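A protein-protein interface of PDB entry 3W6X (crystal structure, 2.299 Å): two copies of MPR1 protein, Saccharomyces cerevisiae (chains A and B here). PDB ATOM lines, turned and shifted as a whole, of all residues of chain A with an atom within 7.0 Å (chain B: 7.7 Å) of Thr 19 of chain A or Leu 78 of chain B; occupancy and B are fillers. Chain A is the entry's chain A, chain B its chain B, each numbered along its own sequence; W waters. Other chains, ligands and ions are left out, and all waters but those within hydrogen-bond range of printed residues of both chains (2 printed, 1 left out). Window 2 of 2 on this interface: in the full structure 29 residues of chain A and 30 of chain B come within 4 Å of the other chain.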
ATOM      1  N   ASN A  16      21.980  22.010  12.491  1.00  0.00           N
ATOM      2  CA  ASN A  16      21.806  22.344  13.915  1.00  0.00           C
ATOM      3  C   ASN A  16      21.559  23.832  14.184  1.00  0.00           C
ATOM      4  O   ASN A  16      22.041  24.400  15.186  1.00  0.00           O
ATOM      5  CB  ASN A  16      23.064  21.925  14.664  1.00  0.00           C
ATOM      6  CG  ASN A  16      23.253  20.421  14.696  1.00  0.00           C
ATOM      7  OD1 ASN A  16      22.325  19.687  14.951  1.00  0.00           O
ATOM      8  ND2 ASN A  16      24.477  19.965  14.460  1.00  0.00           N
ATOM      9  N   GLY A  17      20.846  24.467  13.263  1.00  0.00           N
ATOM     10  CA  GLY A  17      20.495  25.874  13.383  1.00  0.00           C
ATOM     11  C   GLY A  17      19.224  26.153  14.161  1.00  0.00           C
ATOM     12  O   GLY A  17      18.682  25.255  14.770  1.00  0.00           O
ATOM     13  N   PRO A  18      18.740  27.416  14.153  1.00  0.00           N
ATOM     14  CA  PRO A  18      17.485  27.728  14.855  1.00  0.00           C
ATOM     15  C   PRO A  18      16.311  26.883  14.362  1.00  0.00           C
ATOM     16  O   PRO A  18      16.195  26.523  13.185  1.00  0.00           O
ATOM     17  CB  PRO A  18      17.259  29.227  14.568  1.00  0.00           C
ATOM     18  CG  PRO A  18      18.092  29.517  13.362  1.00  0.00           C
ATOM     19  CD  PRO A  18      19.237  28.548  13.353  1.00  0.00           C
ATOM     20  N   THR A  19      15.429  26.551  15.290  1.00  0.00           N
ATOM     21  CA  THR A  19      14.309  25.663  15.032  1.00  0.00           C
ATOM     22  C   THR A  19      13.071  26.416  14.478  1.00  0.00           C
ATOM     23  O   THR A  19      12.303  25.861  13.690  1.00  0.00           O
ATOM     24  CB  THR A  19      13.886  24.973  16.348  1.00  0.00           C
ATOM     25  OG1 THR A  19      14.960  24.188  16.842  1.00  0.00           O
ATOM     26  CG2 THR A  19      12.623  24.054  16.147  1.00  0.00           C
ATOM     27  N   PHE A  20      12.865  27.662  14.899  1.00  0.00           N
ATOM     28  CA  PHE A  20      11.618  28.356  14.548  1.00  0.00           C
ATOM     29  C   PHE A  20      11.749  29.300  13.353  1.00  0.00           C
ATOM     30  O   PHE A  20      10.758  29.775  12.853  1.00  0.00           O
ATOM     31  CB  PHE A  20      11.068  29.111  15.760  1.00  0.00           C
ATOM     32  CG  PHE A  20      10.442  28.220  16.778  1.00  0.00           C
ATOM     33  CD1 PHE A  20      11.214  27.571  17.722  1.00  0.00           C
ATOM     34  CD2 PHE A  20       9.054  27.993  16.770  1.00  0.00           C
ATOM     35  CE1 PHE A  20      10.630  26.736  18.655  1.00  0.00           C
ATOM     36  CE2 PHE A  20       8.453  27.162  17.705  1.00  0.00           C
ATOM     37  CZ  PHE A  20       9.233  26.526  18.648  1.00  0.00           C
ATOM     38  N   PHE A  21      12.962  29.571  12.893  1.00  0.00           N
ATOM     39  CA  PHE A  21      13.150  30.552  11.844  1.00  0.00           C
ATOM     40  C   PHE A  21      14.029  29.974  10.769  1.00  0.00           C
ATOM     41  O   PHE A  21      15.059  29.396  11.073  1.00  0.00           O
ATOM     42  CB  PHE A  21      13.769  31.825  12.430  1.00  0.00           C
ATOM     43  CG  PHE A  21      12.926  32.429  13.494  1.00  0.00           C
ATOM     44  CD1 PHE A  21      11.831  33.217  13.160  1.00  0.00           C
ATOM     45  CD2 PHE A  21      13.149  32.136  14.828  1.00  0.00           C
ATOM     46  CE1 PHE A  21      11.002  33.747  14.156  1.00  0.00           C
ATOM     47  CE2 PHE A  21      12.346  32.662  15.815  1.00  0.00           C
ATOM     48  CZ  PHE A  21      11.258  33.463  15.482  1.00  0.00           C
ATOM     49  N   GLN A  22      13.594  30.125   9.521  1.00  0.00           N
ATOM     50  CA  GLN A  22      14.349  29.744   8.320  1.00  0.00           C
ATOM     51  C   GLN A  22      15.376  30.824   7.955  1.00  0.00           C
ATOM     52  O   GLN A  22      15.222  31.995   8.313  1.00  0.00           O
ATOM     53  CB  GLN A  22      13.361  29.551   7.142  1.00  0.00           C
ATOM     54  N   PRO A 124      23.226  28.032  17.927  1.00  0.00           N
ATOM     55  CA  PRO A 124      22.230  28.333  18.931  1.00  0.00           C
ATOM     56  C   PRO A 124      22.836  28.322  20.301  1.00  0.00           C
ATOM     57  O   PRO A 124      23.579  27.394  20.652  1.00  0.00           O
ATOM     58  CB  PRO A 124      21.229  27.196  18.788  1.00  0.00           C
ATOM     59  CG  PRO A 124      21.419  26.698  17.416  1.00  0.00           C
ATOM     60  CD  PRO A 124      22.897  26.824  17.173  1.00  0.00           C
ATOM     61  N   ALA A 127      18.773  25.528  23.795  1.00  0.00           N
ATOM     62  CA  ALA A 127      17.868  24.537  23.161  1.00  0.00           C
ATOM     63  C   ALA A 127      16.685  25.223  22.392  1.00  0.00           C
ATOM     64  O   ALA A 127      16.495  26.417  22.496  1.00  0.00           O
ATOM     65  CB  ALA A 127      17.359  23.582  24.219  1.00  0.00           C
ATOM     66  N   PRO A 128      15.914  24.469  21.592  1.00  0.00           N
ATOM     67  CA  PRO A 128      15.028  24.996  20.515  1.00  0.00           C
ATOM     68  C   PRO A 128      14.111  26.211  20.759  1.00  0.00           C
ATOM     69  O   PRO A 128      14.031  27.065  19.860  1.00  0.00           O
ATOM     70  CB  PRO A 128      14.197  23.765  20.122  1.00  0.00           C
ATOM     71  CG  PRO A 128      15.249  22.622  20.238  1.00  0.00           C
ATOM     72  CD  PRO A 128      16.002  22.993  21.540  1.00  0.00           C
ATOM     73  N   ARG A 129      13.462  26.327  21.906  1.00  0.00           N
ATOM     74  CA  ARG A 129      12.552  27.476  22.122  1.00  0.00           C
ATOM     75  C   ARG A 129      13.284  28.805  22.258  1.00  0.00           C
ATOM     76  O   ARG A 129      12.699  29.877  22.079  1.00  0.00           O
ATOM     77  CB  ARG A 129      11.662  27.260  23.341  1.00  0.00           C
ATOM     78  CG  ARG A 129      10.501  26.329  23.098  1.00  0.00           C
ATOM     79  CD  ARG A 129       9.694  26.122  24.383  1.00  0.00           C
ATOM     80  NE  ARG A 129       8.645  25.138  24.198  1.00  0.00           N
ATOM     81  CZ  ARG A 129       7.522  25.381  23.522  1.00  0.00           C
ATOM     82  NH1 ARG A 129       7.300  26.564  22.979  1.00  0.00           N
ATOM     83  NH2 ARG A 129       6.627  24.432  23.372  1.00  0.00           N
ATOM     84  N   SER A 131      16.303  29.123  20.543  1.00  0.00           N
ATOM     85  CA  SER A 131      17.355  28.894  19.564  1.00  0.00           C
ATOM     86  C   SER A 131      17.453  30.031  18.550  1.00  0.00           C
ATOM     87  O   SER A 131      18.363  30.034  17.737  1.00  0.00           O
ATOM     88  CB  SER A 131      17.216  27.540  18.849  1.00  0.00           C
ATOM     89  OG  SER A 131      15.989  27.391  18.163  1.00  0.00           O
ATOM     90  N   HIS A 132      16.571  31.026  18.613  1.00  0.00           N
ATOM     91  CA  HIS A 132      16.801  32.250  17.815  1.00  0.00           C
ATOM     92  C   HIS A 132      17.897  33.169  18.421  1.00  0.00           C
ATOM     93  O   HIS A 132      18.241  34.196  17.833  1.00  0.00           O
ATOM     94  CB  HIS A 132      15.501  33.032  17.614  1.00  0.00           C
ATOM     95  CG  HIS A 132      14.909  33.515  18.888  1.00  0.00           C
ATOM     96  ND1 HIS A 132      13.996  32.774  19.606  1.00  0.00           N
ATOM     97  CD2 HIS A 132      15.140  34.635  19.609  1.00  0.00           C
ATOM     98  CE1 HIS A 132      13.674  33.436  20.709  1.00  0.00           C
ATOM     99  NE2 HIS A 132      14.342  34.577  20.720  1.00  0.00           N
ATOM    100  N   TYR A 166      18.782  33.927  12.916  1.00  0.00           N
ATOM    101  CA  TYR A 166      18.867  34.344  14.315  1.00  0.00           C
ATOM    102  C   TYR A 166      18.326  35.746  14.510  1.00  0.00           C
ATOM    103  O   TYR A 166      18.439  36.581  13.600  1.00  0.00           O
ATOM    104  CB  TYR A 166      20.308  34.301  14.760  1.00  0.00           C
ATOM    105  CG  TYR A 166      20.878  32.914  14.775  1.00  0.00           C
ATOM    106  CD1 TYR A 166      20.454  31.982  15.727  1.00  0.00           C
ATOM    107  CD2 TYR A 166      21.872  32.526  13.858  1.00  0.00           C
ATOM    108  CE1 TYR A 166      20.968  30.709  15.759  1.00  0.00           C
ATOM    109  CE2 TYR A 166      22.402  31.223  13.882  1.00  0.00           C
ATOM    110  CZ  TYR A 166      21.929  30.307  14.845  1.00  0.00           C
ATOM    111  OH  TYR A 166      22.408  28.984  14.897  1.00  0.00           O
ATOM    112  N   ASN B  66       9.011  15.222  31.080  1.00  0.00           N
ATOM    113  CA  ASN B  66       8.391  15.326  29.751  1.00  0.00           C
ATOM    114  C   ASN B  66       7.055  16.104  29.760  1.00  0.00           C
ATOM    115  O   ASN B  66       6.738  16.775  28.768  1.00  0.00           O
ATOM    116  CB  ASN B  66       8.244  13.970  29.046  1.00  0.00           C
ATOM    117  CG  ASN B  66       9.541  13.559  28.394  1.00  0.00           C
ATOM    118  OD1 ASN B  66      10.450  14.387  28.276  1.00  0.00           O
ATOM    119  ND2 ASN B  66       9.655  12.299  27.969  1.00  0.00           N
ATOM    120  N   ILE B  69       8.100  19.825  29.856  1.00  0.00           N
ATOM    121  CA  ILE B  69       8.541  20.250  28.559  1.00  0.00           C
ATOM    122  C   ILE B  69       7.328  20.431  27.632  1.00  0.00           C
ATOM    123  O   ILE B  69       7.276  21.394  26.884  1.00  0.00           O
ATOM    124  CB  ILE B  69       9.489  19.246  27.994  1.00  0.00           C
ATOM    125  CG1 ILE B  69      10.800  19.330  28.755  1.00  0.00           C
ATOM    126  CG2 ILE B  69       9.719  19.461  26.461  1.00  0.00           C
ATOM    127  CD1 ILE B  69      11.659  18.188  28.513  1.00  0.00           C
ATOM    128  N   GLU B  70       6.370  19.512  27.686  1.00  0.00           N
ATOM    129  CA  GLU B  70       5.210  19.589  26.793  1.00  0.00           C
ATOM    130  C   GLU B  70       4.343  20.822  27.054  1.00  0.00           C
ATOM    131  O   GLU B  70       3.888  21.450  26.100  1.00  0.00           O
ATOM    132  CB  GLU B  70       4.396  18.304  26.804  1.00  0.00           C
ATOM    133  CG  GLU B  70       5.178  17.162  26.148  1.00  0.00           C
ATOM    134  CD  GLU B  70       5.559  17.429  24.668  1.00  0.00           C
ATOM    135  OE1 GLU B  70       4.636  17.535  23.825  1.00  0.00           O
ATOM    136  OE2 GLU B  70       6.778  17.520  24.343  1.00  0.00           O
ATOM    137  N   SER B  71       4.173  21.203  28.322  1.00  0.00           N
ATOM    138  CA  SER B  71       3.559  22.491  28.644  1.00  0.00           C
ATOM    139  C   SER B  71       4.169  23.625  27.906  1.00  0.00           C
ATOM    140  O   SER B  71       3.468  24.562  27.577  1.00  0.00           O
ATOM    141  CB  SER B  71       3.694  22.826  30.111  1.00  0.00           C
ATOM    142  OG  SER B  71       2.987  21.874  30.861  1.00  0.00           O
ATOM    143  N   GLY B  72       5.492  23.580  27.731  1.00  0.00           N
ATOM    144  CA  GLY B  72       6.205  24.539  26.919  1.00  0.00           C
ATOM    145  C   GLY B  72       6.244  25.946  27.472  1.00  0.00           C
ATOM    146  O   GLY B  72       6.256  26.917  26.700  1.00  0.00           O
ATOM    147  N   TYR B  75      10.895  25.436  30.405  1.00  0.00           N
ATOM    148  CA  TYR B  75      12.185  24.999  29.902  1.00  0.00           C
ATOM    149  C   TYR B  75      12.332  25.276  28.399  1.00  0.00           C
ATOM    150  O   TYR B  75      11.346  25.362  27.672  1.00  0.00           O
ATOM    151  CB  TYR B  75      12.380  23.520  30.148  1.00  0.00           C
ATOM    152  CG  TYR B  75      12.731  23.186  31.558  1.00  0.00           C
ATOM    153  CD1 TYR B  75      11.774  23.170  32.545  1.00  0.00           C
ATOM    154  CD2 TYR B  75      14.041  22.857  31.898  1.00  0.00           C
ATOM    155  CE1 TYR B  75      12.100  22.855  33.860  1.00  0.00           C
ATOM    156  CE2 TYR B  75      14.388  22.523  33.196  1.00  0.00           C
ATOM    157  CZ  TYR B  75      13.427  22.537  34.173  1.00  0.00           C
ATOM    158  OH  TYR B  75      13.820  22.239  35.460  1.00  0.00           O
ATOM    159  N   PRO B  76      13.579  25.417  27.938  1.00  0.00           N
ATOM    160  CA  PRO B  76      13.879  25.757  26.541  1.00  0.00           C
ATOM    161  C   PRO B  76      13.657  24.588  25.583  1.00  0.00           C
ATOM    162  O   PRO B  76      13.633  24.784  24.385  1.00  0.00           O
ATOM    163  CB  PRO B  76      15.373  26.156  26.586  1.00  0.00           C
ATOM    164  CG  PRO B  76      15.908  25.499  27.824  1.00  0.00           C
ATOM    165  CD  PRO B  76      14.781  25.409  28.792  1.00  0.00           C
ATOM    166  N   GLN B  77      13.515  23.384  26.108  1.00  0.00           N
ATOM    167  CA  GLN B  77      13.302  22.203  25.303  1.00  0.00           C
ATOM    168  C   GLN B  77      11.945  22.233  24.580  1.00  0.00           C
ATOM    169  O   GLN B  77      10.952  22.648  25.129  1.00  0.00           O
ATOM    170  CB  GLN B  77      13.325  20.985  26.193  1.00  0.00           C
ATOM    171  CG  GLN B  77      14.711  20.444  26.494  1.00  0.00           C
ATOM    172  CD  GLN B  77      15.401  21.220  27.576  1.00  0.00           C
ATOM    173  OE1 GLN B  77      14.786  21.851  28.400  1.00  0.00           O
ATOM    174  NE2 GLN B  77      16.699  21.186  27.560  1.00  0.00           N
ATOM    175  N   LEU B  78      11.930  21.784  23.338  1.00  0.00           N
ATOM    176  CA  LEU B  78      10.708  21.769  22.568  1.00  0.00           C
ATOM    177  C   LEU B  78      10.087  20.368  22.581  1.00  0.00           C
ATOM    178  O   LEU B  78       8.891  20.225  22.799  1.00  0.00           O
ATOM    179  CB  LEU B  78      10.993  22.196  21.139  1.00  0.00           C
ATOM    180  CG  LEU B  78       9.790  22.035  20.201  1.00  0.00           C
ATOM    181  CD1 LEU B  78       8.520  22.772  20.711  1.00  0.00           C
ATOM    182  CD2 LEU B  78      10.222  22.519  18.822  1.00  0.00           C
ATOM    183  N   HIS B  79      10.915  19.356  22.344  1.00  0.00           N
ATOM    184  CA  HIS B  79      10.474  17.956  22.252  1.00  0.00           C
ATOM    185  C   HIS B  79      10.780  17.163  23.539  1.00  0.00           C
ATOM    186  O   HIS B  79      11.694  17.468  24.275  1.00  0.00           O
ATOM    187  CB  HIS B  79      11.184  17.229  21.099  1.00  0.00           C
ATOM    188  CG  HIS B  79      10.942  17.823  19.750  1.00  0.00           C
ATOM    189  ND1 HIS B  79       9.700  18.259  19.338  1.00  0.00           N
ATOM    190  CD2 HIS B  79      11.780  18.024  18.699  1.00  0.00           C
ATOM    191  CE1 HIS B  79       9.784  18.710  18.099  1.00  0.00           C
ATOM    192  NE2 HIS B  79      11.034  18.581  17.690  1.00  0.00           N
ATOM    193  N   SER B  80       9.975  16.145  23.779  1.00  0.00           N
ATOM    194  CA  SER B  80      10.119  15.267  24.910  1.00  0.00           C
ATOM    195  C   SER B  80      11.456  14.555  24.776  1.00  0.00           C
ATOM    196  O   SER B  80      11.981  14.429  23.685  1.00  0.00           O
ATOM    197  CB  SER B  80       8.945  14.276  24.906  1.00  0.00           C
ATOM    198  OG  SER B  80       7.770  14.942  25.366  1.00  0.00           O
ATOM    199  N   LEU B  81      12.020  14.109  25.878  1.00  0.00           N
ATOM    200  CA  LEU B  81      13.315  13.430  25.847  1.00  0.00           C
ATOM    201  C   LEU B  81      13.077  11.928  25.737  1.00  0.00           C
ATOM    202  O   LEU B  81      12.073  11.423  26.245  1.00  0.00           O
ATOM    203  CB  LEU B  81      14.064  13.694  27.145  1.00  0.00           C
ATOM    204  CG  LEU B  81      14.423  15.121  27.508  1.00  0.00           C
ATOM    205  CD1 LEU B  81      15.456  15.064  28.600  1.00  0.00           C
ATOM    206  CD2 LEU B  81      14.983  15.828  26.344  1.00  0.00           C
ATOM    207  N   ILE B 201      10.405  31.393  22.974  1.00  0.00           N
ATOM    208  CA  ILE B 201       9.119  31.186  22.346  1.00  0.00           C
ATOM    209  C   ILE B 201       8.390  30.131  23.175  1.00  0.00           C
ATOM    210  O   ILE B 201       8.733  28.943  23.151  1.00  0.00           O
ATOM    211  CB  ILE B 201       9.299  30.768  20.872  1.00  0.00           C
ATOM    212  CG1 ILE B 201       9.894  31.963  20.091  1.00  0.00           C
ATOM    213  CG2 ILE B 201       7.960  30.324  20.265  1.00  0.00           C
ATOM    214  CD1 ILE B 201       9.926  31.791  18.563  1.00  0.00           C
ATOM    215  N   ASN B 203       4.794  28.349  24.823  1.00  0.00           N
ATOM    216  CA  ASN B 203       3.438  27.932  24.555  1.00  0.00           C
ATOM    217  C   ASN B 203       2.392  28.855  25.199  1.00  0.00           C
ATOM    218  O   ASN B 203       2.482  29.170  26.381  1.00  0.00           O
ATOM    219  CB  ASN B 203       3.292  26.522  25.103  1.00  0.00           C
ATOM    220  CG  ASN B 203       2.487  25.669  24.223  1.00  0.00           C
ATOM    221  OD1 ASN B 203       1.441  26.098  23.752  1.00  0.00           O
ATOM    222  ND2 ASN B 203       2.960  24.457  23.957  1.00  0.00           N
HETATM  223  O   HOH W   1       7.629  21.994  24.198  1.00  0.00           O
HETATM  224  O   HOH W   2       4.038  22.220  23.377  1.00  0.00           O
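No position is printed for both chains.
Leu 78 of chain B touches Thr 19 of chain A (CD2 to CG2, 3.9 Å).
CD1 of Ile 201 of chain B touches CZ of Phe 21 of chain A (3.7 Å).
Ala 127 of chain A touches Pro 76 of chain B (C to O, 3.7 Å).
Pro 128 of chain A touches Pro 76 of chain B (N to O, 3.6 Å).
Pro 128 of chain A touches Leu 78 of chain B (CB to CB, 3.7 Å).
Arg 129 of chain A touches Gly 72 of chain B (NH2 to CA, 3.6 Å).
CD of Arg 129 of chain A touches O of Tyr 75 of chain B, 3.8 Å away.
NE of Arg 129 of chain A touches O of Gln 77 of chain B (3.5 Å).
Arg 129 of chain A touches Leu 78 of chain B.
Arg 129 of chain A touches Asn 203 of chain B (NH1 to N, 3.6 Å).
The backbone NH of Thr 19 of chain A sits at hydrogen-bond distance from the side-chain hydroxyl of Ser 131 of chain A (3.0 Å).
O of Pro 128 of chain A sits at hydrogen-bond distance from OG of Ser 131 of chain A (2.6 Å).
The backbone carbonyl oxygen of Gly 72 of chain B is in hydrogen-bond range of the backbone NH of Asn 203 of chain B (2.8 Å).
The backbone NH (N) of Arg 129 of chain A is in hydrogen-bond range of the backbone carbonyl oxygen (O) of Pro 76 of chain B (2.9 Å).
The guanidinium group of Arg 129 of chain A is in hydrogen-bond range of the backbone carbonyl oxygen of Ile 201 of chain B (2.8 Å).
Of the 14 printed residues of chain B, 7 touch a printed residue of chain A.
Among the printed residues, 12 pairs touch across the chains.
Water W2 lies within hydrogen-bond range of the side-chain amide nitrogen (ND2) of Asn 203 of chain B (2.6 Å), the backbone carbonyl oxygen (O) of Glu 70 of chain B (2.8 Å) and the guanidinium group (NH2) of Arg 129 of chain A (3.4 Å).
Water W1 lies within hydrogen-bond range of O of Leu 78 of chain B (2.6 Å), NH2 of Arg 129 of chain A (2.8 Å) and O of Ile 69 of chain B (2.8 Å).
Leu 78 of chain B touches just these residues of chain A: Thr 19 (3.9 Å), Pro 128 (3.7 Å) and Arg 129 (3.7 Å).
Printed residues of chain A within 4 Å of Asn 203 of chain B: Arg 129.
Of the printed residues of chain A, Pro 76 of chain B touches Ala 127 (3.7 Å), Pro 128 (3.6 Å) and Arg 129 (2.9 Å).
Of the printed residues of chain B, Ala 127 of chain A touches Pro 76 (3.7 Å).
Of the printed residues of chain A, Gly 72 of chain B touches Arg 129.
Of the printed residues of chain B, Pro 128 of chain A touches Pro 76 (3.6 Å) and Leu 78 (3.7 Å).
Ser 80 of chain B touches none of the printed residues of chain A.
The nearest residue of chain B that does not touch Thr 19 of chain A is His 79 of chain B (5.9 Å).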
